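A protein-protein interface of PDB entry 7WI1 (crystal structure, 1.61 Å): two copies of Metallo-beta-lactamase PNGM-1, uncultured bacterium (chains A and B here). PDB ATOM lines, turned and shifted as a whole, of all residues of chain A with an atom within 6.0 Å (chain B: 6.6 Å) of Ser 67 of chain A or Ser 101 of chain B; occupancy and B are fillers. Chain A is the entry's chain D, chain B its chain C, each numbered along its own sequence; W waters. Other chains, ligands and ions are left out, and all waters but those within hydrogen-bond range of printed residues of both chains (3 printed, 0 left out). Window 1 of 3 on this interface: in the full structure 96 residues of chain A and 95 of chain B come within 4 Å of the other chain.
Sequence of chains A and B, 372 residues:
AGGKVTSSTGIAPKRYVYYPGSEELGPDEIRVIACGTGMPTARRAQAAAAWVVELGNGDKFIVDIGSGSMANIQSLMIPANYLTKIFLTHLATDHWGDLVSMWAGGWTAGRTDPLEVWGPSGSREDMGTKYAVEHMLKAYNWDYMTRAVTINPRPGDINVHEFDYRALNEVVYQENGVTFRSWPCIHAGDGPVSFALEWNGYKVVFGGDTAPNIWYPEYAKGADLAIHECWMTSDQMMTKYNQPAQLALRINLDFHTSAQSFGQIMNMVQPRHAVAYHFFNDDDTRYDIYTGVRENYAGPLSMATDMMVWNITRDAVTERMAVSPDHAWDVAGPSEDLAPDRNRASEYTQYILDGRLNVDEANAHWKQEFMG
The side-chain carboxylate (OD2) of Asp 98 of chain B lies within hydrogen-bond range of the backbone NH (N) of Met 70 of chain B (2.9 Å).
The backbone NH (N) of Ala 48 of chain A sits at hydrogen-bond distance from the backbone carbonyl oxygen (O) of Ser 67 of chain A (3.0 Å).
The backbone carbonyl oxygen (O) of Thr 93 of chain A sits at hydrogen-bond distance from the side-chain hydroxyl (OG) of Ser 67 of chain A, at 3.5 Å.
Among the printed residues, merely in contact across the chains: Pro 40 of chain A with Gly 105 of chain B (3.2 Å), Ala 42 of chain A with Met 70 of chain B (3.7 Å), Ala 42 of chain A with Ala 71 of chain B (3.6 Å), Ser 67 of chain A with Ser 101 of chain B (3.9 Å), Thr 93 of chain A with Val 100 of chain B (3.5 Å) and Thr 93 of chain A with Ala 104 of chain B (3.3 Å).
Of chain B, only Ser 101 (3.9 Å) comes within 4 Å of Ser 67 of chain A.
Of chain A, only Ser 67 comes within 4 Å of Ser 101 of chain B.
Of the printed residues of chain A, Val 100 of chain B touches Thr 93 (3.5 Å).
Of the printed residues of chain A, Ala 104 of chain B touches Thr 93.
Printed residues of chain A within 4 Å of Ala 71 of chain B: Ala 42.
Of the printed residues of chain B, Pro 40 of chain A touches Gly 105.
Of the printed residues of chain A, Gly 105 of chain B touches Pro 40.
Ala 47 of chain A touches none of the printed residues of chain B.
The nearest residue of chain B that does not touch Ser 67 of chain A is Asp 98 of chain B (4.7 Å).
The nearest residue of chain A that does not touch Ser 101 of chain B is Ala 42 of chain A (4.5 Å).
Of the 18 printed residues of chain A, 4 touch a printed residue of chain B.
Of the 16 printed residues of chain B, 6 touch a printed residue of chain A.
Hydrophobic or aromatic side chains of chain B within 4 Å of the printed part of chain A: Met 70, Val 100 and Ala 104.
Along chain B the printed residues that touch a printed residue of chain A span positions 70 to 105.
Positions printed for both chains: 65, 68, 70, 97 and 98.
Of the 6 pairs that touch across the chains among the printed residues, none has its exchanged pair printed and touching as well.
Water W3 lies within hydrogen-bond range of O of Gly 97 of chain B (2.4 Å) and O of Gly 97 of chain A (2.5 Å).
Water W1 lies within hydrogen-bond range of OD1 of Asp 98 of chain B, OD1 of Asp 98 of chain A, N of Gly 68 of chain A and N of Gly 68 of chain B.
Water W2 bridges OG of Ser 67 of chain A (2.7 Å) and OD1 of Asp 98 of chain B (2.9 Å).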
ATOM      1  N   PRO A  40     -20.210  24.417  10.582  1.00  0.00           N
ATOM      2  CA  PRO A  40     -19.346  25.290   9.808  1.00  0.00           C
ATOM      3  C   PRO A  40     -18.254  24.551   9.023  1.00  0.00           C
ATOM      4  O   PRO A  40     -17.584  25.152   8.213  1.00  0.00           O
ATOM      5  CB  PRO A  40     -18.691  26.195  10.858  1.00  0.00           C
ATOM      6  CG  PRO A  40     -19.330  25.856  12.168  1.00  0.00           C
ATOM      7  CD  PRO A  40     -20.062  24.546  12.039  1.00  0.00           C
ATOM      8  N   ALA A  42     -17.533  21.632   6.121  1.00  0.00           N
ATOM      9  CA  ALA A  42     -18.299  21.133   4.962  1.00  0.00           C
ATOM     10  C   ALA A  42     -18.227  19.606   4.809  1.00  0.00           C
ATOM     11  O   ALA A  42     -17.227  18.953   5.224  1.00  0.00           O
ATOM     12  CB  ALA A  42     -17.791  21.782   3.727  1.00  0.00           C
ATOM     13  N   GLN A  46     -24.093  16.624   4.564  1.00  0.00           N
ATOM     14  CA  GLN A  46     -24.867  17.632   5.319  1.00  0.00           C
ATOM     15  C   GLN A  46     -24.390  19.013   4.907  1.00  0.00           C
ATOM     16  O   GLN A  46     -23.322  19.463   5.317  1.00  0.00           O
ATOM     17  CB  GLN A  46     -24.786  17.480   6.829  1.00  0.00           C
ATOM     18  CG  GLN A  46     -25.467  16.230   7.359  1.00  0.00           C
ATOM     19  CD  GLN A  46     -25.242  16.047   8.835  1.00  0.00           C
ATOM     20  OE1 GLN A  46     -24.302  15.349   9.232  1.00  0.00           O
ATOM     21  NE2 GLN A  46     -26.054  16.699   9.661  1.00  0.00           N
ATOM     22  N   ALA A  47     -25.204  19.714   4.156  1.00  0.00           N
ATOM     23  CA  ALA A  47     -25.035  21.172   3.994  1.00  0.00           C
ATOM     24  C   ALA A  47     -25.195  21.867   5.335  1.00  0.00           C
ATOM     25  O   ALA A  47     -25.767  21.270   6.250  1.00  0.00           O
ATOM     26  CB  ALA A  47     -26.039  21.676   2.985  1.00  0.00           C
ATOM     27  N   ALA A  48     -24.770  23.112   5.390  1.00  0.00           N
ATOM     28  CA  ALA A  48     -25.012  23.988   6.550  1.00  0.00           C
ATOM     29  C   ALA A  48     -26.494  24.394   6.575  1.00  0.00           C
ATOM     30  O   ALA A  48     -27.176  24.309   5.554  1.00  0.00           O
ATOM     31  CB  ALA A  48     -24.113  25.174   6.476  1.00  0.00           C
ATOM     32  N   ALA A  49     -26.930  24.820   7.748  1.00  0.00           N
ATOM     33  CA  ALA A  49     -28.333  25.100   8.127  1.00  0.00           C
ATOM     34  C   ALA A  49     -29.111  25.741   6.983  1.00  0.00           C
ATOM     35  O   ALA A  49     -28.760  26.853   6.497  1.00  0.00           O
ATOM     36  CB  ALA A  49     -28.302  26.007   9.324  1.00  0.00           C
ATOM     37  N   ILE A  65     -29.783  29.797   5.043  1.00  0.00           N
ATOM     38  CA  ILE A  65     -29.316  29.404   3.701  1.00  0.00           C
ATOM     39  C   ILE A  65     -27.794  29.258   3.776  1.00  0.00           C
ATOM     40  O   ILE A  65     -27.055  29.971   3.064  1.00  0.00           O
ATOM     41  CB  ILE A  65     -29.860  30.354   2.618  1.00  0.00           C
ATOM     42  CG1 ILE A  65     -29.547  29.859   1.221  1.00  0.00           C
ATOM     43  CG2 ILE A  65     -29.453  31.819   2.790  1.00  0.00           C
ATOM     44  CD1 ILE A  65     -30.446  30.425   0.181  1.00  0.00           C
ATOM     45  N   GLY A  66     -27.369  28.324   4.629  1.00  0.00           N
ATOM     46  CA  GLY A  66     -25.948  28.079   4.919  1.00  0.00           C
ATOM     47  C   GLY A  66     -25.216  27.565   3.677  1.00  0.00           C
ATOM     48  O   GLY A  66     -25.808  26.978   2.763  1.00  0.00           O
ATOM     49  N   SER A  67     -23.902  27.639   3.717  1.00  0.00           N
ATOM     50  CA  SER A  67     -23.033  27.107   2.650  1.00  0.00           C
ATOM     51  C   SER A  67     -23.404  25.667   2.246  1.00  0.00           C
ATOM     52  O   SER A  67     -23.584  24.795   3.161  1.00  0.00           O
ATOM     53  CB  SER A  67     -21.600  27.130   3.145  1.00  0.00           C
ATOM     54  OG  SER A  67     -21.199  28.452   3.478  1.00  0.00           O
ATOM     55  N   GLY A  68     -23.526  25.419   0.946  1.00  0.00           N
ATOM     56  CA  GLY A  68     -23.834  24.084   0.393  1.00  0.00           C
ATOM     57  C   GLY A  68     -25.328  23.791   0.239  1.00  0.00           C
ATOM     58  O   GLY A  68     -25.675  22.810  -0.463  1.00  0.00           O
ATOM     59  N   SER A  69     -26.215  24.553   0.873  1.00  0.00           N
ATOM     60  CA  SER A  69     -27.667  24.267   0.905  1.00  0.00           C
ATOM     61  C   SER A  69     -28.324  24.462  -0.463  1.00  0.00           C
ATOM     62  O   SER A  69     -29.397  23.843  -0.638  1.00  0.00           O
ATOM     63  CB  SER A  69     -28.396  25.007   2.006  1.00  0.00           C
ATOM     64  OG  SER A  69     -28.330  26.404   1.778  1.00  0.00           O
ATOM     65  N   MET A  70     -27.812  25.322  -1.347  1.00  0.00           N
ATOM     66  CA  MET A  70     -28.548  25.597  -2.608  1.00  0.00           C
ATOM     67  C   MET A  70     -28.601  24.352  -3.481  1.00  0.00           C
ATOM     68  O   MET A  70     -29.592  24.204  -4.185  1.00  0.00           O
ATOM     69  CB  MET A  70     -27.944  26.761  -3.396  1.00  0.00           C
ATOM     70  CG  MET A  70     -28.457  28.123  -2.921  1.00  0.00           C
ATOM     71  SD  MET A  70     -30.234  28.319  -3.286  1.00  0.00           S
ATOM     72  CE  MET A  70     -30.233  28.211  -5.055  1.00  0.00           C
ATOM     73  N   THR A  93     -21.499  32.138   8.696  1.00  0.00           N
ATOM     74  CA  THR A  93     -21.404  31.619   7.316  1.00  0.00           C
ATOM     75  C   THR A  93     -22.261  30.368   7.122  1.00  0.00           C
ATOM     76  O   THR A  93     -22.770  30.163   6.040  1.00  0.00           O
ATOM     77  CB  THR A  93     -19.953  31.331   6.919  1.00  0.00           C
ATOM     78  OG1 THR A  93     -19.496  30.143   7.564  1.00  0.00           O
ATOM     79  CG2 THR A  93     -19.088  32.505   7.258  1.00  0.00           C
ATOM     80  N   ASP A  94     -22.454  29.554   8.151  1.00  0.00           N
ATOM     81  CA  ASP A  94     -23.183  28.276   8.047  1.00  0.00           C
ATOM     82  C   ASP A  94     -24.686  28.564   8.105  1.00  0.00           C
ATOM     83  O   ASP A  94     -25.482  27.609   8.076  1.00  0.00           O
ATOM     84  CB  ASP A  94     -22.736  27.218   9.090  1.00  0.00           C
ATOM     85  CG  ASP A  94     -22.926  27.573  10.549  1.00  0.00           C
ATOM     86  OD1 ASP A  94     -22.429  28.661  10.955  1.00  0.00           O
ATOM     87  OD2 ASP A  94     -23.594  26.785  11.320  1.00  0.00           O
ATOM     88  N   HIS A  95     -25.089  29.834   8.136  1.00  0.00           N
ATOM     89  CA  HIS A  95     -26.525  30.203   8.127  1.00  0.00           C
ATOM     90  C   HIS A  95     -26.866  31.111   6.942  1.00  0.00           C
ATOM     91  O   HIS A  95     -28.079  31.259   6.672  1.00  0.00           O
ATOM     92  CB  HIS A  95     -27.006  30.729   9.489  1.00  0.00           C
ATOM     93  CG  HIS A  95     -26.860  29.661  10.532  1.00  0.00           C
ATOM     94  ND1 HIS A  95     -27.929  28.872  10.979  1.00  0.00           N
ATOM     95  CD2 HIS A  95     -25.754  29.116  11.107  1.00  0.00           C
ATOM     96  CE1 HIS A  95     -27.479  28.005  11.856  1.00  0.00           C
ATOM     97  NE2 HIS A  95     -26.169  28.079  11.954  1.00  0.00           N
ATOM     98  N   TRP A  96     -25.919  31.732   6.254  1.00  0.00           N
ATOM     99  CA  TRP A  96     -26.300  32.539   5.059  1.00  0.00           C
ATOM    100  C   TRP A  96     -25.221  32.544   3.963  1.00  0.00           C
ATOM    101  O   TRP A  96     -25.371  33.304   2.974  1.00  0.00           O
ATOM    102  CB  TRP A  96     -26.699  33.980   5.445  1.00  0.00           C
ATOM    103  CG  TRP A  96     -25.568  34.910   5.797  1.00  0.00           C
ATOM    104  CD1 TRP A  96     -24.747  34.833   6.869  1.00  0.00           C
ATOM    105  CD2 TRP A  96     -25.186  36.103   5.089  1.00  0.00           C
ATOM    106  NE1 TRP A  96     -23.849  35.867   6.836  1.00  0.00           N
ATOM    107  CE2 TRP A  96     -24.088  36.661   5.769  1.00  0.00           C
ATOM    108  CE3 TRP A  96     -25.591  36.683   3.895  1.00  0.00           C
ATOM    109  CZ2 TRP A  96     -23.413  37.800   5.324  1.00  0.00           C
ATOM    110  CZ3 TRP A  96     -24.984  37.858   3.492  1.00  0.00           C
ATOM    111  CH2 TRP A  96     -23.894  38.396   4.190  1.00  0.00           C
ATOM    112  N   GLY A  97     -24.209  31.688   4.046  1.00  0.00           N
ATOM    113  CA  GLY A  97     -23.162  31.640   3.005  1.00  0.00           C
ATOM    114  C   GLY A  97     -23.733  31.420   1.619  1.00  0.00           C
ATOM    115  O   GLY A  97     -23.164  31.953   0.658  1.00  0.00           O
ATOM    116  N   ASP A  98     -24.844  30.675   1.448  1.00  0.00           N
ATOM    117  CA  ASP A  98     -25.364  30.422   0.097  1.00  0.00           C
ATOM    118  C   ASP A  98     -26.387  31.494  -0.334  1.00  0.00           C
ATOM    119  O   ASP A  98     -26.969  31.319  -1.396  1.00  0.00           O
ATOM    120  CB  ASP A  98     -25.928  29.006  -0.005  1.00  0.00           C
ATOM    121  CG  ASP A  98     -24.982  28.016  -0.646  1.00  0.00           C
ATOM    122  OD1 ASP A  98     -23.784  28.385  -0.813  1.00  0.00           O
ATOM    123  OD2 ASP A  98     -25.429  26.895  -1.035  1.00  0.00           O
ATOM    124  N   ILE B  65     -12.854  28.401  -6.364  1.00  0.00           N
ATOM    125  CA  ILE B  65     -13.509  27.874  -5.160  1.00  0.00           C
ATOM    126  C   ILE B  65     -14.975  28.300  -5.238  1.00  0.00           C
ATOM    127  O   ILE B  65     -15.517  28.990  -4.376  1.00  0.00           O
ATOM    128  CB  ILE B  65     -12.724  28.263  -3.877  1.00  0.00           C
ATOM    129  CG1 ILE B  65     -13.290  27.545  -2.663  1.00  0.00           C
ATOM    130  CG2 ILE B  65     -12.642  29.777  -3.669  1.00  0.00           C
ATOM    131  CD1 ILE B  65     -12.301  27.507  -1.530  1.00  0.00           C
ATOM    132  N   GLY B  68     -20.347  25.507  -3.376  1.00  0.00           N
ATOM    133  CA  GLY B  68     -20.560  24.085  -3.160  1.00  0.00           C
ATOM    134  C   GLY B  68     -19.293  23.260  -3.156  1.00  0.00           C
ATOM    135  O   GLY B  68     -19.368  22.116  -2.777  1.00  0.00           O
ATOM    136  N   MET B  70     -16.547  23.390  -1.364  1.00  0.00           N
ATOM    137  CA  MET B  70     -15.835  23.113  -0.098  1.00  0.00           C
ATOM    138  C   MET B  70     -16.185  21.723   0.436  1.00  0.00           C
ATOM    139  O   MET B  70     -15.326  21.094   1.069  1.00  0.00           O
ATOM    140  CB  MET B  70     -16.143  24.164   0.958  1.00  0.00           C
ATOM    141  CG  MET B  70     -15.159  24.182   2.096  1.00  0.00           C
ATOM    142  SD  MET B  70     -13.445  24.642   1.517  1.00  0.00           S
ATOM    143  CE  MET B  70     -12.488  23.457   2.453  1.00  0.00           C
ATOM    144  N   ALA B  71     -17.392  21.226   0.226  1.00  0.00           N
ATOM    145  CA  ALA B  71     -17.710  19.841   0.619  1.00  0.00           C
ATOM    146  C   ALA B  71     -16.784  18.812  -0.052  1.00  0.00           C
ATOM    147  O   ALA B  71     -16.444  17.785   0.552  1.00  0.00           O
ATOM    148  CB  ALA B  71     -19.138  19.526   0.330  1.00  0.00           C
ATOM    149  N   GLY B  97     -17.554  31.647  -4.734  1.00  0.00           N
ATOM    150  CA  GLY B  97     -18.645  31.655  -3.748  1.00  0.00           C
ATOM    151  C   GLY B  97     -18.279  30.932  -2.474  1.00  0.00           C
ATOM    152  O   GLY B  97     -18.848  31.291  -1.460  1.00  0.00           O
ATOM    153  N   ASP B  98     -17.383  29.936  -2.503  1.00  0.00           N
ATOM    154  CA  ASP B  98     -17.072  29.138  -1.301  1.00  0.00           C
ATOM    155  C   ASP B  98     -15.785  29.684  -0.663  1.00  0.00           C
ATOM    156  O   ASP B  98     -15.331  29.032   0.287  1.00  0.00           O
ATOM    157  CB  ASP B  98     -17.051  27.638  -1.593  1.00  0.00           C
ATOM    158  CG  ASP B  98     -18.320  26.899  -1.190  1.00  0.00           C
ATOM    159  OD1 ASP B  98     -19.379  27.580  -0.999  1.00  0.00           O
ATOM    160  OD2 ASP B  98     -18.275  25.648  -1.119  1.00  0.00           O
ATOM    161  N   LEU B  99     -15.262  30.828  -1.095  1.00  0.00           N
ATOM    162  CA  LEU B  99     -14.078  31.337  -0.342  1.00  0.00           C
ATOM    163  C   LEU B  99     -14.481  31.543   1.104  1.00  0.00           C
ATOM    164  O   LEU B  99     -13.682  31.279   1.985  1.00  0.00           O
ATOM    165  CB  LEU B  99     -13.543  32.636  -0.957  1.00  0.00           C
ATOM    166  CG  LEU B  99     -12.314  33.217  -0.253  1.00  0.00           C
ATOM    167  CD1 LEU B  99     -11.166  32.251  -0.362  1.00  0.00           C
ATOM    168  CD2 LEU B  99     -11.947  34.584  -0.834  1.00  0.00           C
ATOM    169  N   VAL B 100     -15.686  32.041   1.330  1.00  0.00           N
ATOM    170  CA  VAL B 100     -16.128  32.329   2.725  1.00  0.00           C
ATOM    171  C   VAL B 100     -16.204  31.022   3.506  1.00  0.00           C
ATOM    172  O   VAL B 100     -15.950  31.052   4.716  1.00  0.00           O
ATOM    173  CB  VAL B 100     -17.459  33.085   2.794  1.00  0.00           C
ATOM    174  CG1 VAL B 100     -18.607  32.284   2.284  1.00  0.00           C
ATOM    175  CG2 VAL B 100     -17.730  33.538   4.209  1.00  0.00           C
ATOM    176  N   SER B 101     -16.562  29.885   2.900  1.00  0.00           N
ATOM    177  CA  SER B 101     -16.636  28.582   3.618  1.00  0.00           C
ATOM    178  C   SER B 101     -15.214  28.090   3.959  1.00  0.00           C
ATOM    179  O   SER B 101     -15.003  27.543   5.023  1.00  0.00           O
ATOM    180  CB  SER B 101     -17.425  27.580   2.785  1.00  0.00           C
ATOM    181  OG  SER B 101     -17.453  26.306   3.422  1.00  0.00           O
ATOM    182  N   MET B 102     -14.254  28.254   3.064  1.00  0.00           N
ATOM    183  CA  MET B 102     -12.829  27.966   3.375  1.00  0.00           C
ATOM    184  C   MET B 102     -12.364  28.889   4.515  1.00  0.00           C
ATOM    185  O   MET B 102     -11.693  28.421   5.409  1.00  0.00           O
ATOM    186  CB  MET B 102     -11.926  28.129   2.160  1.00  0.00           C
ATOM    187  CG  MET B 102     -10.448  27.991   2.483  1.00  0.00           C
ATOM    188  SD  MET B 102     -10.038  26.386   3.075  1.00  0.00           S
ATOM    189  CE  MET B 102      -9.678  25.671   1.469  1.00  0.00           C
ATOM    190  N   TRP B 103     -12.687  30.166   4.432  1.00  0.00           N
ATOM    191  CA  TRP B 103     -12.242  31.160   5.445  1.00  0.00           C
ATOM    192  C   TRP B 103     -12.779  30.747   6.832  1.00  0.00           C
ATOM    193  O   TRP B 103     -12.001  30.561   7.771  1.00  0.00           O
ATOM    194  CB  TRP B 103     -12.731  32.533   4.986  1.00  0.00           C
ATOM    195  CG  TRP B 103     -12.583  33.617   5.998  1.00  0.00           C
ATOM    196  CD1 TRP B 103     -11.445  34.260   6.359  1.00  0.00           C
ATOM    197  CD2 TRP B 103     -13.663  34.210   6.722  1.00  0.00           C
ATOM    198  NE1 TRP B 103     -11.739  35.225   7.296  1.00  0.00           N
ATOM    199  CE2 TRP B 103     -13.092  35.242   7.498  1.00  0.00           C
ATOM    200  CE3 TRP B 103     -15.046  34.026   6.730  1.00  0.00           C
ATOM    201  CZ2 TRP B 103     -13.855  36.041   8.329  1.00  0.00           C
ATOM    202  CZ3 TRP B 103     -15.809  34.835   7.548  1.00  0.00           C
ATOM    203  CH2 TRP B 103     -15.217  35.821   8.335  1.00  0.00           C
ATOM    204  N   ALA B 104     -14.087  30.628   6.963  1.00  0.00           N
ATOM    205  CA  ALA B 104     -14.743  30.312   8.253  1.00  0.00           C
ATOM    206  C   ALA B 104     -14.483  28.867   8.675  1.00  0.00           C
ATOM    207  O   ALA B 104     -14.097  28.634   9.837  1.00  0.00           O
ATOM    208  CB  ALA B 104     -16.233  30.599   8.166  1.00  0.00           C
ATOM    209  N   GLY B 105     -14.734  27.908   7.791  1.00  0.00           N
ATOM    210  CA  GLY B 105     -14.620  26.475   8.120  1.00  0.00           C
ATOM    211  C   GLY B 105     -13.175  26.127   8.401  1.00  0.00           C
ATOM    212  O   GLY B 105     -12.939  25.504   9.414  1.00  0.00           O
ATOM    213  N   GLY B 106     -12.231  26.645   7.590  1.00  0.00           N
ATOM    214  CA  GLY B 106     -10.776  26.438   7.788  1.00  0.00           C
ATOM    215  C   GLY B 106     -10.307  26.987   9.132  1.00  0.00           C
ATOM    216  O   GLY B 106      -9.459  26.391   9.762  1.00  0.00           O
ATOM    217  N   TRP B 107     -10.833  28.151   9.562  1.00  0.00           N
ATOM    218  CA  TRP B 107     -10.559  28.791  10.874  1.00  0.00           C
ATOM    219  C   TRP B 107     -11.104  27.895  11.988  1.00  0.00           C
ATOM    220  O   TRP B 107     -10.371  27.685  12.963  1.00  0.00           O
ATOM    221  CB  TRP B 107     -11.161  30.203  10.865  1.00  0.00           C
ATOM    222  CG  TRP B 107     -10.713  31.161  11.923  1.00  0.00           C
ATOM    223  CD1 TRP B 107      -9.802  31.000  12.933  1.00  0.00           C
ATOM    224  CD2 TRP B 107     -11.201  32.491  12.061  1.00  0.00           C
ATOM    225  NE1 TRP B 107      -9.766  32.123  13.718  1.00  0.00           N
ATOM    226  CE2 TRP B 107     -10.620  33.053  13.224  1.00  0.00           C
ATOM    227  CE3 TRP B 107     -12.132  33.243  11.361  1.00  0.00           C
ATOM    228  CZ2 TRP B 107     -10.886  34.366  13.603  1.00  0.00           C
ATOM    229  CZ3 TRP B 107     -12.392  34.541  11.742  1.00  0.00           C
ATOM    230  CH2 TRP B 107     -11.800  35.079  12.878  1.00  0.00           C
ATOM    231  N   ARG B 111      -6.924  26.189  11.140  1.00  0.00           N
ATOM    232  CA  ARG B 111      -5.952  26.991  10.343  1.00  0.00           C
ATOM    233  C   ARG B 111      -5.305  28.055  11.252  1.00  0.00           C
ATOM    234  O   ARG B 111      -6.040  28.709  12.050  1.00  0.00           O
ATOM    235  CB  ARG B 111      -6.600  27.688   9.135  1.00  0.00           C
ATOM    236  CG  ARG B 111      -5.623  28.493   8.310  1.00  0.00           C
ATOM    237  CD  ARG B 111      -6.215  29.175   7.087  1.00  0.00           C
ATOM    238  NE  ARG B 111      -7.203  30.186   7.452  1.00  0.00           N
ATOM    239  CZ  ARG B 111      -8.533  30.114   7.242  1.00  0.00           C
ATOM    240  NH1 ARG B 111      -9.095  29.079   6.647  1.00  0.00           N
ATOM    241  NH2 ARG B 111      -9.271  31.121   7.661  1.00  0.00           N
HETATM  242  O   HOH W   1     -21.789  26.815  -0.995  1.00  0.00           O
HETATM  243  O   HOH W   2     -20.281  29.369   1.126  1.00  0.00           O
HETATM  244  O   HOH W   3     -20.938  31.970  -0.453  1.00  0.00           O
